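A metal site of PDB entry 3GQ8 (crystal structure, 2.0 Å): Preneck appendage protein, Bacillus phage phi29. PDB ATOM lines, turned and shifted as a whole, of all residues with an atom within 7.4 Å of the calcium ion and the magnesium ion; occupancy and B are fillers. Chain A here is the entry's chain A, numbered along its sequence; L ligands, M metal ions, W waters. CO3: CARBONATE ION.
Water W1 bridges OG1 of Thr 201 (2.8 Å) and NE2 of His 203 (3.1 Å).
The magnesium ion is bound by OD2 of Asp 230 (2.0 Å), water W1 (2.0 Å), water W2 (2.0 Å), OE1 of Glu 228 (2.1 Å), O1 of the ligand (2.2 Å) and O3 of the ligand (2.4 Å).
The magnesium ion has six donor atoms within binding distance.
His 203 touches the magnesium ion (NE2 to MG, 3.4 Å).
NZ of Lys 253 touches the magnesium ion (3.9 Å).
Within 4 Å of the magnesium ion: Asp 198, His 203, Glu 228, Asp 230 and Lys 253.
The calcium ion is bound by OD2 of Asp 197 (2.3 Å), O of Asn 223 (2.3 Å), OE2 of Glu 228 (2.3 Å), OD1 of Asp 198 (2.4 Å), OD2 of Asp 198 (2.5 Å), O1 of the ligand (2.5 Å) and O2 of the ligand (2.6 Å).
The calcium ion has seven donor atoms within binding distance.
Merely in contact with the calcium ion: Asn 225 (3.9 Å).
OD2 of Asp 230 sits close to NE2 of His 203 (3.3 Å).
O of Thr 202 sits at hydrogen-bond distance from N of Asp 230 (2.9 Å).
ND2 of Asn 225 lies close to OE2 of Glu 228, at 2.8 Å.
O of Glu 228 sits at hydrogen-bond distance from N of Thr 202 (3.0 Å).
The side-chain carboxylate of Asp 198 lies close to the backbone NH of Asn 225 (2.8 Å).
N of Asp 198 lies within hydrogen-bond range of ND1 of His 158 (3.2 Å).
The backbone NH (N) of Gly 199 is in hydrogen-bond range of the backbone carbonyl oxygen (O) of Asn 225 (3.0 Å).
N of Asp 231 is in hydrogen-bond range of O of Lys 253, at 3.4 Å.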
ATOM      1  N   HIS A 158      -4.634  -3.937  -2.789  1.00  0.00           N
ATOM      2  CA  HIS A 158      -4.890  -2.489  -2.681  1.00  0.00           C
ATOM      3  C   HIS A 158      -4.612  -1.750  -3.985  1.00  0.00           C
ATOM      4  O   HIS A 158      -3.957  -2.274  -4.890  1.00  0.00           O
ATOM      5  CB  HIS A 158      -4.007  -1.832  -1.600  1.00  0.00           C
ATOM      6  CG  HIS A 158      -3.903  -2.607  -0.320  1.00  0.00           C
ATOM      7  ND1 HIS A 158      -4.985  -2.857   0.485  1.00  0.00           N
ATOM      8  CD2 HIS A 158      -2.830  -3.130   0.315  1.00  0.00           C
ATOM      9  CE1 HIS A 158      -4.589  -3.537   1.553  1.00  0.00           C
ATOM     10  NE2 HIS A 158      -3.286  -3.711   1.475  1.00  0.00           N
ATOM     11  N   ASP A 161      -0.332   1.066  -1.810  1.00  0.00           N
ATOM     12  CA  ASP A 161       0.031   0.628  -0.461  1.00  0.00           C
ATOM     13  C   ASP A 161       1.423   1.138  -0.103  1.00  0.00           C
ATOM     14  O   ASP A 161       2.406   0.877  -0.816  1.00  0.00           O
ATOM     15  CB  ASP A 161       0.008  -0.900  -0.387  1.00  0.00           C
ATOM     16  CG  ASP A 161       0.321  -1.476   1.012  1.00  0.00           C
ATOM     17  OD1 ASP A 161       0.599  -2.700   1.079  1.00  0.00           O
ATOM     18  OD2 ASP A 161       0.266  -0.754   2.032  1.00  0.00           O
ATOM     19  N   TYR A 169       3.296  -8.296   6.107  1.00  0.00           N
ATOM     20  CA  TYR A 169       3.083  -7.282   7.132  1.00  0.00           C
ATOM     21  C   TYR A 169       3.584  -7.871   8.450  1.00  0.00           C
ATOM     22  O   TYR A 169       3.249  -9.010   8.764  1.00  0.00           O
ATOM     23  CB  TYR A 169       1.609  -6.907   7.261  1.00  0.00           C
ATOM     24  CG  TYR A 169       1.030  -6.265   6.020  1.00  0.00           C
ATOM     25  CD1 TYR A 169      -0.099  -6.814   5.397  1.00  0.00           C
ATOM     26  CD2 TYR A 169       1.606  -5.133   5.459  1.00  0.00           C
ATOM     27  CE1 TYR A 169      -0.633  -6.245   4.246  1.00  0.00           C
ATOM     28  CE2 TYR A 169       1.085  -4.546   4.310  1.00  0.00           C
ATOM     29  CZ  TYR A 169      -0.037  -5.105   3.715  1.00  0.00           C
ATOM     30  OH  TYR A 169      -0.563  -4.538   2.579  1.00  0.00           O
ATOM     31  N   TYR A 171       3.715  -8.411  12.452  1.00  0.00           N
ATOM     32  CA  TYR A 171       2.838  -8.316  13.612  1.00  0.00           C
ATOM     33  C   TYR A 171       3.663  -8.529  14.876  1.00  0.00           C
ATOM     34  O   TYR A 171       3.796  -9.653  15.360  1.00  0.00           O
ATOM     35  CB  TYR A 171       1.680  -9.327  13.491  1.00  0.00           C
ATOM     36  CG  TYR A 171       0.832  -9.090  12.257  1.00  0.00           C
ATOM     37  CD1 TYR A 171       1.017  -9.872  11.117  1.00  0.00           C
ATOM     38  CD2 TYR A 171      -0.108  -8.059  12.212  1.00  0.00           C
ATOM     39  CE1 TYR A 171       0.258  -9.650   9.958  1.00  0.00           C
ATOM     40  CE2 TYR A 171      -0.884  -7.831  11.056  1.00  0.00           C
ATOM     41  CZ  TYR A 171      -0.683  -8.632   9.939  1.00  0.00           C
ATOM     42  OH  TYR A 171      -1.431  -8.421   8.798  1.00  0.00           O
ATOM     43  N   GLY A 196      -9.446  -5.262  -3.997  1.00  0.00           N
ATOM     44  CA  GLY A 196      -9.825  -6.403  -3.158  1.00  0.00           C
ATOM     45  C   GLY A 196      -9.827  -6.091  -1.676  1.00  0.00           C
ATOM     46  O   GLY A 196     -10.560  -6.712  -0.898  1.00  0.00           O
ATOM     47  N   ASP A 197      -8.973  -5.161  -1.262  1.00  0.00           N
ATOM     48  CA  ASP A 197      -8.906  -4.795   0.139  1.00  0.00           C
ATOM     49  C   ASP A 197      -9.163  -3.300   0.249  1.00  0.00           C
ATOM     50  O   ASP A 197     -10.330  -2.906   0.309  1.00  0.00           O
ATOM     51  CB  ASP A 197      -7.556  -5.195   0.739  1.00  0.00           C
ATOM     52  CG  ASP A 197      -7.610  -5.353   2.247  1.00  0.00           C
ATOM     53  OD1 ASP A 197      -6.768  -6.103   2.804  1.00  0.00           O
ATOM     54  OD2 ASP A 197      -8.477  -4.737   2.897  1.00  0.00           O
ATOM     55  N   ASP A 198      -8.120  -2.480   0.201  1.00  0.00           N
ATOM     56  CA  ASP A 198      -8.265  -1.018   0.378  1.00  0.00           C
ATOM     57  C   ASP A 198      -7.839  -0.194  -0.833  1.00  0.00           C
ATOM     58  O   ASP A 198      -7.057  -0.649  -1.663  1.00  0.00           O
ATOM     59  CB  ASP A 198      -7.513  -0.555   1.630  1.00  0.00           C
ATOM     60  CG  ASP A 198      -7.877  -1.364   2.842  1.00  0.00           C
ATOM     61  OD1 ASP A 198      -9.084  -1.441   3.180  1.00  0.00           O
ATOM     62  OD2 ASP A 198      -6.972  -1.961   3.462  1.00  0.00           O
ATOM     63  N   GLY A 199      -8.359   1.019  -0.939  1.00  0.00           N
ATOM     64  CA  GLY A 199      -7.992   1.876  -2.060  1.00  0.00           C
ATOM     65  C   GLY A 199      -6.593   2.422  -1.884  1.00  0.00           C
ATOM     66  O   GLY A 199      -5.701   2.168  -2.694  1.00  0.00           O
ATOM     67  N   THR A 201      -3.708   2.855   1.274  1.00  0.00           N
ATOM     68  CA  THR A 201      -3.435   2.421   2.638  1.00  0.00           C
ATOM     69  C   THR A 201      -1.991   2.642   3.055  1.00  0.00           C
ATOM     70  O   THR A 201      -1.095   2.650   2.205  1.00  0.00           O
ATOM     71  CB  THR A 201      -3.854   0.915   2.832  1.00  0.00           C
ATOM     72  OG1 THR A 201      -3.591   0.514   4.174  1.00  0.00           O
ATOM     73  CG2 THR A 201      -3.111   0.011   1.886  1.00  0.00           C
ATOM     74  N   THR A 202      -1.765   2.848   4.347  1.00  0.00           N
ATOM     75  CA  THR A 202      -0.399   2.983   4.891  1.00  0.00           C
ATOM     76  C   THR A 202      -0.166   1.966   5.999  1.00  0.00           C
ATOM     77  O   THR A 202      -1.080   1.660   6.778  1.00  0.00           O
ATOM     78  CB  THR A 202      -0.112   4.428   5.430  1.00  0.00           C
ATOM     79  OG1 THR A 202      -0.934   4.698   6.568  1.00  0.00           O
ATOM     80  CG2 THR A 202      -0.421   5.468   4.373  1.00  0.00           C
ATOM     81  N   HIS A 203       1.049   1.429   6.055  1.00  0.00           N
ATOM     82  CA  HIS A 203       1.474   0.536   7.133  1.00  0.00           C
ATOM     83  C   HIS A 203       2.886   0.891   7.576  1.00  0.00           C
ATOM     84  O   HIS A 203       3.760   1.081   6.746  1.00  0.00           O
ATOM     85  CB  HIS A 203       1.549  -0.927   6.670  1.00  0.00           C
ATOM     86  CG  HIS A 203       0.268  -1.478   6.114  1.00  0.00           C
ATOM     87  ND1 HIS A 203      -0.101  -1.293   4.801  1.00  0.00           N
ATOM     88  CD2 HIS A 203      -0.683  -2.261   6.672  1.00  0.00           C
ATOM     89  CE1 HIS A 203      -1.243  -1.913   4.576  1.00  0.00           C
ATOM     90  NE2 HIS A 203      -1.622  -2.501   5.694  1.00  0.00           N
ATOM     91  N   ALA A 222     -15.416  -7.420   2.687  1.00  0.00           N
ATOM     92  CA  ALA A 222     -14.775  -7.577   3.992  1.00  0.00           C
ATOM     93  C   ALA A 222     -14.355  -6.180   4.565  1.00  0.00           C
ATOM     94  O   ALA A 222     -15.115  -5.218   4.447  1.00  0.00           O
ATOM     95  CB  ALA A 222     -13.568  -8.524   3.882  1.00  0.00           C
ATOM     96  N   ASN A 223     -13.184  -6.098   5.211  1.00  0.00           N
ATOM     97  CA  ASN A 223     -12.690  -4.820   5.752  1.00  0.00           C
ATOM     98  C   ASN A 223     -12.114  -3.950   4.620  1.00  0.00           C
ATOM     99  O   ASN A 223     -10.898  -3.715   4.567  1.00  0.00           O
ATOM    100  CB  ASN A 223     -11.651  -5.026   6.864  1.00  0.00           C
ATOM    101  CG  ASN A 223     -11.324  -3.731   7.628  1.00  0.00           C
ATOM    102  OD1 ASN A 223     -12.204  -2.935   7.924  1.00  0.00           O
ATOM    103  ND2 ASN A 223     -10.039  -3.522   7.943  1.00  0.00           N
ATOM    104  N   CYS A 224     -12.988  -3.518   3.714  1.00  0.00           N
ATOM    105  CA  CYS A 224     -12.566  -2.899   2.453  1.00  0.00           C
ATOM    106  C   CYS A 224     -12.807  -1.405   2.514  1.00  0.00           C
ATOM    107  O   CYS A 224     -13.941  -0.940   2.364  1.00  0.00           O
ATOM    108  CB  CYS A 224     -13.320  -3.524   1.289  1.00  0.00           C
ATOM    109  SG  CYS A 224     -13.001  -5.292   1.117  1.00  0.00           S
ATOM    110  N   ASN A 225     -11.720  -0.667   2.714  1.00  0.00           N
ATOM    111  CA  ASN A 225     -11.836   0.733   3.116  1.00  0.00           C
ATOM    112  C   ASN A 225     -11.314   1.654   2.029  1.00  0.00           C
ATOM    113  O   ASN A 225     -10.466   1.274   1.235  1.00  0.00           O
ATOM    114  CB  ASN A 225     -11.089   0.981   4.442  1.00  0.00           C
ATOM    115  CG  ASN A 225     -11.651   0.138   5.596  1.00  0.00           C
ATOM    116  OD1 ASN A 225     -12.861   0.071   5.786  1.00  0.00           O
ATOM    117  ND2 ASN A 225     -10.769  -0.499   6.348  1.00  0.00           N
ATOM    118  N   GLU A 228      -7.145   3.498   4.360  1.00  0.00           N
ATOM    119  CA  GLU A 228      -6.907   2.770   5.590  1.00  0.00           C
ATOM    120  C   GLU A 228      -5.529   3.097   6.145  1.00  0.00           C
ATOM    121  O   GLU A 228      -4.523   2.697   5.581  1.00  0.00           O
ATOM    122  CB  GLU A 228      -7.072   1.255   5.398  1.00  0.00           C
ATOM    123  CG  GLU A 228      -7.182   0.515   6.731  1.00  0.00           C
ATOM    124  CD  GLU A 228      -7.203  -0.983   6.577  1.00  0.00           C
ATOM    125  OE1 GLU A 228      -6.187  -1.631   6.946  1.00  0.00           O
ATOM    126  OE2 GLU A 228      -8.226  -1.529   6.090  1.00  0.00           O
ATOM    127  N   ILE A 229      -5.522   3.829   7.247  1.00  0.00           N
ATOM    128  CA  ILE A 229      -4.268   4.199   7.928  1.00  0.00           C
ATOM    129  C   ILE A 229      -4.089   3.108   8.992  1.00  0.00           C
ATOM    130  O   ILE A 229      -4.683   3.149  10.066  1.00  0.00           O
ATOM    131  CB  ILE A 229      -4.379   5.619   8.528  1.00  0.00           C
ATOM    132  CG1 ILE A 229      -4.833   6.629   7.457  1.00  0.00           C
ATOM    133  CG2 ILE A 229      -3.073   6.038   9.222  1.00  0.00           C
ATOM    134  CD1 ILE A 229      -4.095   6.539   6.068  1.00  0.00           C
ATOM    135  N   ASP A 230      -3.277   2.118   8.649  1.00  0.00           N
ATOM    136  CA  ASP A 230      -3.302   0.825   9.342  1.00  0.00           C
ATOM    137  C   ASP A 230      -2.090   0.646  10.248  1.00  0.00           C
ATOM    138  O   ASP A 230      -1.306   1.578  10.442  1.00  0.00           O
ATOM    139  CB  ASP A 230      -3.337  -0.287   8.293  1.00  0.00           C
ATOM    140  CG  ASP A 230      -3.895  -1.614   8.834  1.00  0.00           C
ATOM    141  OD1 ASP A 230      -4.366  -1.684   9.997  1.00  0.00           O
ATOM    142  OD2 ASP A 230      -3.869  -2.595   8.064  1.00  0.00           O
ATOM    143  N   ASP A 231      -1.979  -0.558  10.816  1.00  0.00           N
ATOM    144  CA  ASP A 231      -0.829  -1.029  11.597  1.00  0.00           C
ATOM    145  C   ASP A 231       0.451  -0.209  11.444  1.00  0.00           C
ATOM    146  O   ASP A 231       1.050  -0.191  10.371  1.00  0.00           O
ATOM    147  CB  ASP A 231      -0.463  -2.483  11.205  1.00  0.00           C
ATOM    148  CG  ASP A 231      -1.624  -3.488  11.404  1.00  0.00           C
ATOM    149  OD1 ASP A 231      -2.561  -3.226  12.194  1.00  0.00           O
ATOM    150  OD2 ASP A 231      -1.566  -4.566  10.768  1.00  0.00           O
ATOM    151  N   GLU A 251     -10.441   4.663   7.671  1.00  0.00           N
ATOM    152  CA  GLU A 251     -10.187   3.851   8.847  1.00  0.00           C
ATOM    153  C   GLU A 251      -8.801   4.183   9.405  1.00  0.00           C
ATOM    154  O   GLU A 251      -7.852   4.318   8.652  1.00  0.00           O
ATOM    155  CB  GLU A 251     -10.290   2.347   8.524  1.00  0.00           C
ATOM    156  CG  GLU A 251      -9.817   1.446   9.681  1.00  0.00           C
ATOM    157  CD  GLU A 251     -10.139  -0.027   9.467  1.00  0.00           C
ATOM    158  OE1 GLU A 251      -9.254  -0.749   8.969  1.00  0.00           O
ATOM    159  OE2 GLU A 251     -11.280  -0.432   9.777  1.00  0.00           O
ATOM    160  N   LYS A 253      -6.506   2.495  12.348  1.00  0.00           N
ATOM    161  CA  LYS A 253      -6.546   1.345  13.250  1.00  0.00           C
ATOM    162  C   LYS A 253      -5.242   0.590  13.389  1.00  0.00           C
ATOM    163  O   LYS A 253      -4.234   0.958  12.794  1.00  0.00           O
ATOM    164  CB  LYS A 253      -7.628   0.362  12.790  1.00  0.00           C
ATOM    165  CG  LYS A 253      -7.199  -0.584  11.680  1.00  0.00           C
ATOM    166  CD  LYS A 253      -8.054  -1.872  11.771  1.00  0.00           C
ATOM    167  CE  LYS A 253      -7.453  -3.035  10.991  1.00  0.00           C
ATOM    168  NZ  LYS A 253      -7.061  -2.642   9.618  1.00  0.00           N
ATOM    169  N   HIS A 255      -4.499  -4.029  13.965  1.00  0.00           N
ATOM    170  CA  HIS A 255      -4.898  -5.357  14.455  1.00  0.00           C
ATOM    171  C   HIS A 255      -4.414  -5.536  15.872  1.00  0.00           C
ATOM    172  O   HIS A 255      -3.600  -4.732  16.360  1.00  0.00           O
ATOM    173  CB  HIS A 255      -4.287  -6.422  13.560  1.00  0.00           C
ATOM    174  CG  HIS A 255      -4.833  -6.386  12.166  1.00  0.00           C
ATOM    175  ND1 HIS A 255      -4.208  -5.719  11.141  1.00  0.00           N
ATOM    176  CD2 HIS A 255      -5.984  -6.878  11.655  1.00  0.00           C
ATOM    177  CE1 HIS A 255      -4.927  -5.834  10.046  1.00  0.00           C
ATOM    178  NE2 HIS A 255      -6.020  -6.529  10.324  1.00  0.00           N
ATOM    179  N   ARG A 281     -10.224   2.619  15.514  1.00  0.00           N
ATOM    180  CA  ARG A 281     -10.328   1.439  16.405  1.00  0.00           C
ATOM    181  C   ARG A 281      -8.978   0.767  16.592  1.00  0.00           C
ATOM    182  O   ARG A 281      -8.061   0.980  15.810  1.00  0.00           O
ATOM    183  CB  ARG A 281     -11.346   0.428  15.834  1.00  0.00           C
ATOM    184  CG  ARG A 281     -10.990  -0.110  14.432  1.00  0.00           C
ATOM    185  CD  ARG A 281     -12.231  -0.673  13.740  1.00  0.00           C
ATOM    186  NE  ARG A 281     -11.945  -1.220  12.420  1.00  0.00           N
ATOM    187  CZ  ARG A 281     -11.929  -2.526  12.132  1.00  0.00           C
ATOM    188  NH1 ARG A 281     -12.209  -3.435  13.080  1.00  0.00           N
ATOM    189  NH2 ARG A 281     -11.671  -2.923  10.903  1.00  0.00           N
HETATM  190  C   CO3 L   1      -7.002  -4.632   6.586  1.00  0.00           C
HETATM  191  O1  CO3 L   1      -6.484  -4.253   5.460  1.00  0.00           O
HETATM  192  O2  CO3 L   1      -8.242  -4.987   6.619  1.00  0.00           O
HETATM  193  O3  CO3 L   1      -6.273  -4.612   7.660  1.00  0.00           O
HETATM  194 CA    CA M   1      -8.624  -3.320   4.671  1.00  0.00          CA
HETATM  195 MG    MG M   2      -4.845  -3.186   6.417  1.00  0.00          MG
HETATM  196  O   HOH W   1      -4.527  -2.115   4.709  1.00  0.00           O
HETATM  197  O   HOH W   2      -3.377  -4.543   5.971  1.00  0.00           O
